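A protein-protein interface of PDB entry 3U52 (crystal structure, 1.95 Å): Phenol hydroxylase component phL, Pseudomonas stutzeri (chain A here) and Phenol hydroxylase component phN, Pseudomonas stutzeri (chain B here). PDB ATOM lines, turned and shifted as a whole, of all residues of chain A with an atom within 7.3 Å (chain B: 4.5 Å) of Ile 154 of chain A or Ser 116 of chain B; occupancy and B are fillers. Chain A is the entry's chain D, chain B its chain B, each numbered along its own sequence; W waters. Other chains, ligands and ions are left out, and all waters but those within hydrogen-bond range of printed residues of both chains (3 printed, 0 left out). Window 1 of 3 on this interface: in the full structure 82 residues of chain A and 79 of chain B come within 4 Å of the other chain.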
ATOM      1  N   TYR A  81      -4.029  -1.268   9.745  1.00  0.00           N
ATOM      2  CA  TYR A  81      -4.520  -2.636   9.605  1.00  0.00           C
ATOM      3  C   TYR A  81      -5.164  -3.182  10.893  1.00  0.00           C
ATOM      4  O   TYR A  81      -6.247  -3.741  10.849  1.00  0.00           O
ATOM      5  CB  TYR A  81      -3.410  -3.588   9.157  1.00  0.00           C
ATOM      6  CG  TYR A  81      -3.863  -5.001   9.012  1.00  0.00           C
ATOM      7  CD1 TYR A  81      -4.331  -5.484   7.785  1.00  0.00           C
ATOM      8  CD2 TYR A  81      -3.813  -5.885  10.091  1.00  0.00           C
ATOM      9  CE1 TYR A  81      -4.718  -6.795   7.635  1.00  0.00           C
ATOM     10  CE2 TYR A  81      -4.201  -7.234   9.934  1.00  0.00           C
ATOM     11  CZ  TYR A  81      -4.650  -7.658   8.707  1.00  0.00           C
ATOM     12  OH  TYR A  81      -5.004  -8.956   8.541  1.00  0.00           O
ATOM     13  N   TYR A  84      -8.563  -1.637  11.704  1.00  0.00           N
ATOM     14  CA  TYR A  84      -9.526  -2.143  10.737  1.00  0.00           C
ATOM     15  C   TYR A  84     -10.009  -3.547  11.082  1.00  0.00           C
ATOM     16  O   TYR A  84     -11.234  -3.788  11.158  1.00  0.00           O
ATOM     17  CB  TYR A  84      -8.971  -1.988   9.279  1.00  0.00           C
ATOM     18  CG  TYR A  84      -9.717  -2.851   8.267  1.00  0.00           C
ATOM     19  CD1 TYR A  84     -10.949  -2.463   7.793  1.00  0.00           C
ATOM     20  CD2 TYR A  84      -9.184  -4.059   7.830  1.00  0.00           C
ATOM     21  CE1 TYR A  84     -11.657  -3.256   6.860  1.00  0.00           C
ATOM     22  CE2 TYR A  84      -9.888  -4.879   6.907  1.00  0.00           C
ATOM     23  CZ  TYR A  84     -11.120  -4.444   6.429  1.00  0.00           C
ATOM     24  OH  TYR A  84     -11.855  -5.220   5.524  1.00  0.00           O
ATOM     25  N   ASN A 134     -15.618  -4.676  -5.269  1.00  0.00           N
ATOM     26  CA  ASN A 134     -14.347  -5.293  -4.867  1.00  0.00           C
ATOM     27  C   ASN A 134     -13.268  -5.092  -5.951  1.00  0.00           C
ATOM     28  O   ASN A 134     -12.164  -4.638  -5.652  1.00  0.00           O
ATOM     29  CB  ASN A 134     -14.548  -6.787  -4.529  1.00  0.00           C
ATOM     30  CG  ASN A 134     -13.264  -7.567  -4.452  1.00  0.00           C
ATOM     31  OD1 ASN A 134     -12.926  -8.296  -5.386  1.00  0.00           O
ATOM     32  ND2 ASN A 134     -12.539  -7.448  -3.324  1.00  0.00           N
ATOM     33  N   MET A 135     -13.590  -5.410  -7.210  1.00  0.00           N
ATOM     34  CA  MET A 135     -12.587  -5.329  -8.281  1.00  0.00           C
ATOM     35  C   MET A 135     -12.134  -3.872  -8.526  1.00  0.00           C
ATOM     36  O   MET A 135     -10.921  -3.600  -8.704  1.00  0.00           O
ATOM     37  CB  MET A 135     -13.093  -5.982  -9.569  1.00  0.00           C
ATOM     38  CG  MET A 135     -13.402  -7.476  -9.441  1.00  0.00           C
ATOM     39  SD  MET A 135     -14.070  -8.027 -11.005  1.00  0.00           S
ATOM     40  CE  MET A 135     -12.579  -7.889 -12.023  1.00  0.00           C
ATOM     41  N   ASN A 137     -12.121  -1.332  -6.383  1.00  0.00           N
ATOM     42  CA  ASN A 137     -11.294  -0.886  -5.268  1.00  0.00           C
ATOM     43  C   ASN A 137      -9.942  -1.551  -5.206  1.00  0.00           C
ATOM     44  O   ASN A 137      -9.003  -0.900  -4.753  1.00  0.00           O
ATOM     45  CB  ASN A 137     -12.084  -1.046  -3.936  1.00  0.00           C
ATOM     46  CG  ASN A 137     -13.181   0.019  -3.808  1.00  0.00           C
ATOM     47  OD1 ASN A 137     -14.415  -0.268  -3.793  1.00  0.00           O
ATOM     48  ND2 ASN A 137     -12.738   1.253  -3.714  1.00  0.00           N
ATOM     49  N   ALA A 138      -9.819  -2.827  -5.616  1.00  0.00           N
ATOM     50  CA  ALA A 138      -8.495  -3.401  -5.843  1.00  0.00           C
ATOM     51  C   ALA A 138      -7.691  -2.632  -6.877  1.00  0.00           C
ATOM     52  O   ALA A 138      -6.479  -2.399  -6.684  1.00  0.00           O
ATOM     53  CB  ALA A 138      -8.560  -4.891  -6.244  1.00  0.00           C
ATOM     54  N   LYS A 139      -8.330  -2.297  -7.991  1.00  0.00           N
ATOM     55  CA  LYS A 139      -7.689  -1.391  -8.993  1.00  0.00           C
ATOM     56  C   LYS A 139      -7.170  -0.069  -8.374  1.00  0.00           C
ATOM     57  O   LYS A 139      -6.005   0.294  -8.567  1.00  0.00           O
ATOM     58  CB  LYS A 139      -8.614  -1.182 -10.208  1.00  0.00           C
ATOM     59  CG  LYS A 139      -8.015  -0.482 -11.469  1.00  0.00           C
ATOM     60  CD  LYS A 139      -8.492   0.965 -11.495  1.00  0.00           C
ATOM     61  CE  LYS A 139      -8.492   1.679 -12.893  1.00  0.00           C
ATOM     62  NZ  LYS A 139      -7.213   1.589 -13.583  1.00  0.00           N
ATOM     63  N   ILE A 140      -8.006   0.632  -7.613  1.00  0.00           N
ATOM     64  CA  ILE A 140      -7.577   1.909  -7.016  1.00  0.00           C
ATOM     65  C   ILE A 140      -6.432   1.651  -6.055  1.00  0.00           C
ATOM     66  O   ILE A 140      -5.430   2.378  -6.072  1.00  0.00           O
ATOM     67  CB  ILE A 140      -8.787   2.671  -6.352  1.00  0.00           C
ATOM     68  CG1 ILE A 140      -9.857   2.956  -7.383  1.00  0.00           C
ATOM     69  CG2 ILE A 140      -8.391   3.952  -5.623  1.00  0.00           C
ATOM     70  CD1 ILE A 140     -11.274   2.937  -6.791  1.00  0.00           C
ATOM     71  N   ALA A 141      -6.529   0.602  -5.230  1.00  0.00           N
ATOM     72  CA  ALA A 141      -5.505   0.383  -4.214  1.00  0.00           C
ATOM     73  C   ALA A 141      -4.117   0.180  -4.900  1.00  0.00           C
ATOM     74  O   ALA A 141      -3.045   0.552  -4.350  1.00  0.00           O
ATOM     75  CB  ALA A 141      -5.884  -0.758  -3.266  1.00  0.00           C
ATOM     76  N   GLY A 142      -4.144  -0.384  -6.100  1.00  0.00           N
ATOM     77  CA  GLY A 142      -2.936  -0.606  -6.868  1.00  0.00           C
ATOM     78  C   GLY A 142      -2.440   0.642  -7.592  1.00  0.00           C
ATOM     79  O   GLY A 142      -1.254   0.707  -7.932  1.00  0.00           O
ATOM     80  N   ASP A 143      -3.334   1.598  -7.866  1.00  0.00           N
ATOM     81  CA  ASP A 143      -3.007   2.814  -8.677  1.00  0.00           C
ATOM     82  C   ASP A 143      -2.740   4.101  -7.914  1.00  0.00           C
ATOM     83  O   ASP A 143      -1.968   4.929  -8.397  1.00  0.00           O
ATOM     84  CB  ASP A 143      -4.114   3.122  -9.697  1.00  0.00           C
ATOM     85  CG  ASP A 143      -4.083   2.176 -10.900  1.00  0.00           C
ATOM     86  OD1 ASP A 143      -3.207   1.310 -10.960  1.00  0.00           O
ATOM     87  OD2 ASP A 143      -4.928   2.321 -11.793  1.00  0.00           O
ATOM     88  N   VAL A 149      -4.426   6.856   0.993  1.00  0.00           N
ATOM     89  CA  VAL A 149      -5.496   6.636   0.009  1.00  0.00           C
ATOM     90  C   VAL A 149      -5.592   5.171  -0.393  1.00  0.00           C
ATOM     91  O   VAL A 149      -6.677   4.609  -0.382  1.00  0.00           O
ATOM     92  CB  VAL A 149      -5.270   7.537  -1.224  1.00  0.00           C
ATOM     93  CG1 VAL A 149      -6.302   7.221  -2.319  1.00  0.00           C
ATOM     94  CG2 VAL A 149      -5.291   9.033  -0.782  1.00  0.00           C
ATOM     95  N   SER A 150      -4.473   4.524  -0.723  1.00  0.00           N
ATOM     96  CA  SER A 150      -4.570   3.113  -1.141  1.00  0.00           C
ATOM     97  C   SER A 150      -5.067   2.165  -0.005  1.00  0.00           C
ATOM     98  O   SER A 150      -5.822   1.209  -0.253  1.00  0.00           O
ATOM     99  CB  SER A 150      -3.240   2.637  -1.728  1.00  0.00           C
ATOM    100  OG  SER A 150      -2.222   2.756  -0.716  1.00  0.00           O
ATOM    101  N   GLN A 151      -4.683   2.436   1.252  1.00  0.00           N
ATOM    102  CA  GLN A 151      -5.178   1.537   2.303  1.00  0.00           C
ATOM    103  C   GLN A 151      -6.692   1.669   2.458  1.00  0.00           C
ATOM    104  O   GLN A 151      -7.350   0.706   2.695  1.00  0.00           O
ATOM    105  CB  GLN A 151      -4.422   1.687   3.622  1.00  0.00           C
ATOM    106  CG  GLN A 151      -4.828   2.846   4.470  1.00  0.00           C
ATOM    107  CD  GLN A 151      -4.056   2.874   5.817  1.00  0.00           C
ATOM    108  OE1 GLN A 151      -3.628   3.939   6.285  1.00  0.00           O
ATOM    109  NE2 GLN A 151      -3.919   1.722   6.431  1.00  0.00           N
ATOM    110  N   MET A 152      -7.254   2.859   2.293  1.00  0.00           N
ATOM    111  CA  MET A 152      -8.719   2.998   2.468  1.00  0.00           C
ATOM    112  C   MET A 152      -9.443   2.233   1.393  1.00  0.00           C
ATOM    113  O   MET A 152     -10.513   1.689   1.597  1.00  0.00           O
ATOM    114  CB  MET A 152      -9.101   4.476   2.409  1.00  0.00           C
ATOM    115  CG  MET A 152      -8.622   5.291   3.628  1.00  0.00           C
ATOM    116  SD  MET A 152      -9.445   6.934   3.678  1.00  0.00           S
ATOM    117  CE  MET A 152      -8.841   7.810   2.246  1.00  0.00           C
ATOM    118  N   HIS A 153      -8.844   2.165   0.210  1.00  0.00           N
ATOM    119  CA  HIS A 153      -9.428   1.352  -0.872  1.00  0.00           C
ATOM    120  C   HIS A 153      -9.279  -0.183  -0.765  1.00  0.00           C
ATOM    121  O   HIS A 153     -10.213  -0.905  -1.105  1.00  0.00           O
ATOM    122  CB  HIS A 153      -8.959   1.895  -2.235  1.00  0.00           C
ATOM    123  CG  HIS A 153      -9.506   3.243  -2.518  1.00  0.00           C
ATOM    124  ND1 HIS A 153      -8.875   4.397  -2.117  1.00  0.00           N
ATOM    125  CD2 HIS A 153     -10.650   3.629  -3.134  1.00  0.00           C
ATOM    126  CE1 HIS A 153      -9.601   5.440  -2.479  1.00  0.00           C
ATOM    127  NE2 HIS A 153     -10.675   5.005  -3.106  1.00  0.00           N
ATOM    128  N   ILE A 154      -8.152  -0.696  -0.264  1.00  0.00           N
ATOM    129  CA  ILE A 154      -8.088  -2.130  -0.045  1.00  0.00           C
ATOM    130  C   ILE A 154      -9.069  -2.552   1.083  1.00  0.00           C
ATOM    131  O   ILE A 154      -9.727  -3.576   0.958  1.00  0.00           O
ATOM    132  CB  ILE A 154      -6.654  -2.701   0.213  1.00  0.00           C
ATOM    133  CG1 ILE A 154      -6.683  -4.233   0.160  1.00  0.00           C
ATOM    134  CG2 ILE A 154      -6.126  -2.302   1.600  1.00  0.00           C
ATOM    135  CD1 ILE A 154      -6.232  -4.871  -1.115  1.00  0.00           C
ATOM    136  N   TYR A 155      -9.164  -1.769   2.160  1.00  0.00           N
ATOM    137  CA  TYR A 155     -10.116  -2.082   3.254  1.00  0.00           C
ATOM    138  C   TYR A 155     -11.557  -2.126   2.708  1.00  0.00           C
ATOM    139  O   TYR A 155     -12.305  -3.072   2.950  1.00  0.00           O
ATOM    140  CB  TYR A 155     -10.014  -1.027   4.376  1.00  0.00           C
ATOM    141  CG  TYR A 155      -8.661  -1.001   5.076  1.00  0.00           C
ATOM    142  CD1 TYR A 155      -8.206   0.141   5.716  1.00  0.00           C
ATOM    143  CD2 TYR A 155      -7.844  -2.157   5.117  1.00  0.00           C
ATOM    144  CE1 TYR A 155      -6.945   0.161   6.349  1.00  0.00           C
ATOM    145  CE2 TYR A 155      -6.595  -2.140   5.754  1.00  0.00           C
ATOM    146  CZ  TYR A 155      -6.187  -0.971   6.370  1.00  0.00           C
ATOM    147  OH  TYR A 155      -4.958  -0.877   6.947  1.00  0.00           O
ATOM    148  N   THR A 156     -11.926  -1.122   1.937  1.00  0.00           N
ATOM    149  CA  THR A 156     -13.288  -1.081   1.393  1.00  0.00           C
ATOM    150  C   THR A 156     -13.546  -2.219   0.366  1.00  0.00           C
ATOM    151  O   THR A 156     -14.633  -2.816   0.364  1.00  0.00           O
ATOM    152  CB  THR A 156     -13.704   0.370   0.945  1.00  0.00           C
ATOM    153  OG1 THR A 156     -15.139   0.528   1.083  1.00  0.00           O
ATOM    154  CG2 THR A 156     -13.322   0.638  -0.451  1.00  0.00           C
ATOM    155  N   GLY A 157     -12.559  -2.548  -0.465  1.00  0.00           N
ATOM    156  CA  GLY A 157     -12.709  -3.667  -1.422  1.00  0.00           C
ATOM    157  C   GLY A 157     -12.874  -5.007  -0.723  1.00  0.00           C
ATOM    158  O   GLY A 157     -13.656  -5.861  -1.160  1.00  0.00           O
ATOM    159  N   MET A 158     -12.138  -5.209   0.367  1.00  0.00           N
ATOM    160  CA  MET A 158     -12.313  -6.416   1.160  1.00  0.00           C
ATOM    161  C   MET A 158     -13.684  -6.451   1.876  1.00  0.00           C
ATOM    162  O   MET A 158     -14.315  -7.493   1.912  1.00  0.00           O
ATOM    163  CB  MET A 158     -11.120  -6.632   2.118  1.00  0.00           C
ATOM    164  CG  MET A 158      -9.749  -6.910   1.389  1.00  0.00           C
ATOM    165  SD  MET A 158      -9.873  -7.878  -0.174  1.00  0.00           S
ATOM    166  CE  MET A 158      -9.672  -6.595  -1.482  1.00  0.00           C
ATOM    167  N   ASP A 159     -14.160  -5.313   2.367  1.00  0.00           N
ATOM    168  CA  ASP A 159     -15.531  -5.189   2.913  1.00  0.00           C
ATOM    169  C   ASP A 159     -16.574  -5.575   1.856  1.00  0.00           C
ATOM    170  O   ASP A 159     -17.537  -6.242   2.166  1.00  0.00           O
ATOM    171  CB  ASP A 159     -15.801  -3.742   3.279  1.00  0.00           C
ATOM    172  CG  ASP A 159     -14.965  -3.251   4.466  1.00  0.00           C
ATOM    173  OD1 ASP A 159     -14.444  -4.093   5.224  1.00  0.00           O
ATOM    174  OD2 ASP A 159     -14.824  -2.012   4.624  1.00  0.00           O
ATOM    175  N   ARG A 160     -16.367  -5.151   0.601  1.00  0.00           N
ATOM    176  CA  ARG A 160     -17.347  -5.446  -0.480  1.00  0.00           C
ATOM    177  C   ARG A 160     -17.424  -6.933  -0.742  1.00  0.00           C
ATOM    178  O   ARG A 160     -18.510  -7.451  -0.973  1.00  0.00           O
ATOM    179  CB  ARG A 160     -17.061  -4.684  -1.812  1.00  0.00           C
ATOM    180  CG  ARG A 160     -16.794  -3.210  -1.707  1.00  0.00           C
ATOM    181  CD  ARG A 160     -17.861  -2.453  -0.880  1.00  0.00           C
ATOM    182  NE  ARG A 160     -19.138  -2.310  -1.574  1.00  0.00           N
ATOM    183  CZ  ARG A 160     -19.487  -1.272  -2.334  1.00  0.00           C
ATOM    184  NH1 ARG A 160     -18.667  -0.229  -2.491  1.00  0.00           N
ATOM    185  NH2 ARG A 160     -20.674  -1.280  -2.931  1.00  0.00           N
ATOM    186  N   PHE B 112       2.364  -5.309  -1.134  1.00  0.00           N
ATOM    187  CA  PHE B 112       0.974  -4.830  -0.944  1.00  0.00           C
ATOM    188  C   PHE B 112       0.435  -4.206  -2.235  1.00  0.00           C
ATOM    189  O   PHE B 112      -0.634  -4.595  -2.712  1.00  0.00           O
ATOM    190  CB  PHE B 112       0.896  -3.810   0.217  1.00  0.00           C
ATOM    191  CG  PHE B 112      -0.258  -2.837   0.110  1.00  0.00           C
ATOM    192  CD1 PHE B 112      -1.584  -3.297  -0.013  1.00  0.00           C
ATOM    193  CD2 PHE B 112      -0.017  -1.440   0.135  1.00  0.00           C
ATOM    194  CE1 PHE B 112      -2.647  -2.397  -0.101  1.00  0.00           C
ATOM    195  CE2 PHE B 112      -1.059  -0.551   0.064  1.00  0.00           C
ATOM    196  CZ  PHE B 112      -2.385  -1.033  -0.061  1.00  0.00           C
ATOM    197  N   GLN B 113       1.155  -3.211  -2.760  1.00  0.00           N
ATOM    198  CA  GLN B 113       0.807  -2.631  -4.087  1.00  0.00           C
ATOM    199  C   GLN B 113       0.723  -3.605  -5.280  1.00  0.00           C
ATOM    200  O   GLN B 113      -0.224  -3.521  -6.051  1.00  0.00           O
ATOM    201  CB  GLN B 113       1.765  -1.489  -4.440  1.00  0.00           C
ATOM    202  CG  GLN B 113       1.809  -0.443  -3.319  1.00  0.00           C
ATOM    203  CD  GLN B 113       2.641   0.744  -3.685  1.00  0.00           C
ATOM    204  OE1 GLN B 113       3.853   0.659  -3.739  1.00  0.00           O
ATOM    205  NE2 GLN B 113       1.985   1.860  -3.967  1.00  0.00           N
ATOM    206  N   GLY B 114       1.751  -4.442  -5.450  1.00  0.00           N
ATOM    207  CA  GLY B 114       1.851  -5.447  -6.514  1.00  0.00           C
ATOM    208  C   GLY B 114       0.719  -6.450  -6.440  1.00  0.00           C
ATOM    209  O   GLY B 114       0.100  -6.774  -7.464  1.00  0.00           O
ATOM    210  N   TYR B 115       0.423  -6.951  -5.248  1.00  0.00           N
ATOM    211  CA  TYR B 115      -0.666  -7.946  -5.141  1.00  0.00           C
ATOM    212  C   TYR B 115      -2.076  -7.320  -5.314  1.00  0.00           C
ATOM    213  O   TYR B 115      -3.009  -7.991  -5.793  1.00  0.00           O
ATOM    214  CB  TYR B 115      -0.570  -8.759  -3.826  1.00  0.00           C
ATOM    215  CG  TYR B 115       0.446  -9.895  -3.869  1.00  0.00           C
ATOM    216  CD1 TYR B 115       1.720  -9.736  -3.295  1.00  0.00           C
ATOM    217  CD2 TYR B 115       0.143 -11.123  -4.490  1.00  0.00           C
ATOM    218  CE1 TYR B 115       2.683 -10.775  -3.345  1.00  0.00           C
ATOM    219  CE2 TYR B 115       1.084 -12.148  -4.542  1.00  0.00           C
ATOM    220  CZ  TYR B 115       2.344 -11.969  -3.968  1.00  0.00           C
ATOM    221  OH  TYR B 115       3.259 -12.995  -4.009  1.00  0.00           O
ATOM    222  N   SER B 116      -2.235  -6.060  -4.930  1.00  0.00           N
ATOM    223  CA  SER B 116      -3.516  -5.342  -5.138  1.00  0.00           C
ATOM    224  C   SER B 116      -3.794  -5.266  -6.663  1.00  0.00           C
ATOM    225  O   SER B 116      -4.897  -5.564  -7.148  1.00  0.00           O
ATOM    226  CB  SER B 116      -3.450  -3.908  -4.579  1.00  0.00           C
ATOM    227  OG  SER B 116      -3.366  -3.832  -3.143  1.00  0.00           O
ATOM    228  N   LYS B 117      -2.757  -4.917  -7.408  1.00  0.00           N
ATOM    229  CA  LYS B 117      -2.880  -4.758  -8.828  1.00  0.00           C
ATOM    230  C   LYS B 117      -3.179  -6.087  -9.468  1.00  0.00           C
ATOM    231  O   LYS B 117      -4.089  -6.203 -10.240  1.00  0.00           O
ATOM    232  CB  LYS B 117      -1.632  -4.123  -9.417  1.00  0.00           C
ATOM    233  CG  LYS B 117      -1.766  -4.030 -10.961  1.00  0.00           C
ATOM    234  CD  LYS B 117      -0.738  -3.202 -11.599  1.00  0.00           C
ATOM    235  CE  LYS B 117      -0.717  -3.500 -13.121  1.00  0.00           C
ATOM    236  NZ  LYS B 117      -1.960  -2.984 -13.719  1.00  0.00           N
ATOM    237  N   VAL B 118      -2.425  -7.102  -9.100  1.00  0.00           N
ATOM    238  CA  VAL B 118      -2.585  -8.442  -9.637  1.00  0.00           C
ATOM    239  C   VAL B 118      -3.912  -9.087  -9.169  1.00  0.00           C
ATOM    240  O   VAL B 118      -4.516  -9.915  -9.891  1.00  0.00           O
ATOM    241  CB  VAL B 118      -1.239  -9.225  -9.324  1.00  0.00           C
ATOM    242  CG1 VAL B 118      -1.441 -10.347  -8.407  1.00  0.00           C
ATOM    243  CG2 VAL B 118      -0.449  -9.597 -10.607  1.00  0.00           C
ATOM    244  N   GLY B 119      -4.430  -8.686  -8.014  1.00  0.00           N
ATOM    245  CA  GLY B 119      -5.781  -9.113  -7.612  1.00  0.00           C
ATOM    246  C   GLY B 119      -6.922  -8.455  -8.409  1.00  0.00           C
ATOM    247  O   GLY B 119      -8.109  -8.646  -8.095  1.00  0.00           O
ATOM    248  N   ARG B 120      -6.579  -7.599  -9.391  1.00  0.00           N
ATOM    249  CA  ARG B 120      -7.585  -7.046 -10.308  1.00  0.00           C
ATOM    250  C   ARG B 120      -7.462  -7.668 -11.725  1.00  0.00           C
ATOM    251  O   ARG B 120      -8.451  -7.833 -12.440  1.00  0.00           O
ATOM    252  CB  ARG B 120      -7.477  -5.505 -10.340  1.00  0.00           C
ATOM    253  CG  ARG B 120      -8.229  -4.805 -11.494  1.00  0.00           C
ATOM    254  CD  ARG B 120      -9.742  -4.960 -11.389  1.00  0.00           C
ATOM    255  NE  ARG B 120     -10.428  -4.400 -12.551  1.00  0.00           N
ATOM    256  CZ  ARG B 120     -10.460  -4.956 -13.767  1.00  0.00           C
ATOM    257  NH1 ARG B 120      -9.870  -6.148 -14.040  1.00  0.00           N
ATOM    258  NH2 ARG B 120     -11.122  -4.313 -14.715  1.00  0.00           N
ATOM    259  N   GLN B 132      -5.702 -10.869  -3.415  1.00  0.00           N
ATOM    260  CA  GLN B 132      -6.191  -9.771  -2.610  1.00  0.00           C
ATOM    261  C   GLN B 132      -5.967 -10.004  -1.139  1.00  0.00           C
ATOM    262  O   GLN B 132      -5.585  -9.094  -0.449  1.00  0.00           O
ATOM    263  CB  GLN B 132      -7.696  -9.555  -2.835  1.00  0.00           C
ATOM    264  CG  GLN B 132      -8.018  -9.099  -4.236  1.00  0.00           C
ATOM    265  CD  GLN B 132      -9.512  -8.940  -4.441  1.00  0.00           C
ATOM    266  OE1 GLN B 132     -10.296  -9.042  -3.477  1.00  0.00           O
ATOM    267  NE2 GLN B 132      -9.924  -8.717  -5.685  1.00  0.00           N
ATOM    268  N   ALA B 135      -2.472  -9.347  -0.619  1.00  0.00           N
ATOM    269  CA  ALA B 135      -2.160  -7.904  -0.631  1.00  0.00           C
ATOM    270  C   ALA B 135      -2.402  -7.319   0.775  1.00  0.00           C
ATOM    271  O   ALA B 135      -1.561  -6.593   1.278  1.00  0.00           O
ATOM    272  CB  ALA B 135      -3.000  -7.158  -1.635  1.00  0.00           C
ATOM    273  N   ILE B 136      -3.562  -7.608   1.355  1.00  0.00           N
ATOM    274  CA  ILE B 136      -3.865  -7.008   2.652  1.00  0.00           C
ATOM    275  C   ILE B 136      -2.943  -7.566   3.780  1.00  0.00           C
ATOM    276  O   ILE B 136      -2.569  -6.829   4.698  1.00  0.00           O
ATOM    277  CB  ILE B 136      -5.357  -7.056   2.998  1.00  0.00           C
ATOM    278  CG1 ILE B 136      -5.640  -6.035   4.119  1.00  0.00           C
ATOM    279  CG2 ILE B 136      -5.804  -8.514   3.437  1.00  0.00           C
ATOM    280  CD1 ILE B 136      -7.165  -5.738   4.374  1.00  0.00           C
ATOM    281  N   LEU B 139       0.205  -5.541   3.569  1.00  0.00           N
ATOM    282  CA  LEU B 139       0.021  -4.247   4.218  1.00  0.00           C
ATOM    283  C   LEU B 139       0.168  -4.385   5.754  1.00  0.00           C
ATOM    284  O   LEU B 139       0.808  -3.567   6.419  1.00  0.00           O
ATOM    285  CB  LEU B 139      -1.353  -3.672   3.911  1.00  0.00           C
ATOM    286  CG  LEU B 139      -1.745  -2.356   4.581  1.00  0.00           C
ATOM    287  CD1 LEU B 139      -0.755  -1.171   4.264  1.00  0.00           C
ATOM    288  CD2 LEU B 139      -3.176  -2.019   4.152  1.00  0.00           C
HETATM  289  O   HOH W   1       0.490   3.139  -1.619  1.00  0.00           O
HETATM  290  O   HOH W   2      -0.759   1.920  -4.333  1.00  0.00           O
HETATM  291  O   HOH W   3      -2.298   0.403 -13.255  1.00  0.00           O
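The side-chain amide oxygen of Gln 132 of chain B is in hydrogen-bond range of the side-chain amide nitrogen of Asn 134 of chain A. The side-chain amide oxygen of Gln 132 of chain B lies close to the side-chain sulfur of Met 158 of chain A, at 3.5 Å.
The backbone carbonyl oxygen (O) of Phe 112 of chain B lies within hydrogen-bond range of the side-chain hydroxyl (OG) of Ser 116 of chain B (2.9 Å). The side-chain hydroxyl of Tyr 155 of chain A lies within hydrogen-bond range of the backbone NH of Tyr 81 of chain A, at 3.0 Å. The side-chain hydroxyl (OH) of Tyr 84 of chain A is in hydrogen-bond range of the backbone carbonyl oxygen (O) of Tyr 155 of chain A, at 3.4 Å. ND2 of Asn 134 of chain A lies within hydrogen-bond range of O of Gly 157 of chain A, 2.9 Å away. NZ of Lys 139 of chain A is in salt-bridge range of OD2 of Asp 143 of chain A, at 3.0 Å. NE2 of Gln 151 of chain A is in hydrogen-bond range of OH of Tyr 155 of chain A (2.8 Å).
Ile 136 of chain B touches Tyr 81 of chain A. Tyr 84 of chain A touches Ile 136 of chain B (CE2 to CD1, 3.8 Å). O of Met 135 of chain A touches CD of Arg 120 of chain B, at 3.2 Å. Ser 116 of chain B touches Ala 138 of chain A (O to O, 3.6 Å). Ser 116 of chain B touches Gly 142 of chain A. Ser 150 of chain A touches Phe 112 of chain B. CE1 of Phe 112 of chain B touches CG2 of Ile 154 of chain A, at 3.9 Å. OG of Ser 116 of chain B touches CD1 of Ile 154 of chain A, 3.7 Å away. Ala 135 of chain B touches Ile 154 of chain A. Ile 154 of chain A touches Leu 139 of chain B.
Printed residues of chain B within 4 Å of Ile 154 of chain A: Phe 112, Ser 116, Ala 135 and Leu 139. Ser 116 of chain B touches four residues of chain A. Of the printed residues of chain B, Tyr 155 of chain A touches Ile 136 (3.7 Å) and Leu 139 (3.5 Å). Of the printed residues of chain B, Ala 141 of chain A touches Ser 116. Ile 140 of chain A touches none of the printed residues of chain B. The nearest printed residue of chain A that does not touch Gln 132 of chain B is Ala 138 of chain A (4.1 Å).
Along chain A the printed residues that touch a printed residue of chain B span positions 81 to 158. Among the printed residues, 17 pairs touch across the chains.
Water W3 lies within hydrogen-bond range of the side-chain carboxylate of Asp 143 of chain A (2.6 Å) and the side-chain amino group of Lys 117 of chain B (3.4 Å). Water W2 bridges the backbone carbonyl oxygen of Ala 141 of chain A (2.7 Å) and the side-chain amide nitrogen of Gln 113 of chain B (2.8 Å). Water W1 lies within hydrogen-bond range of the side-chain hydroxyl of Ser 150 of chain A (2.9 Å) and the side-chain amide nitrogen of Gln 113 of chain B (3.1 Å).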
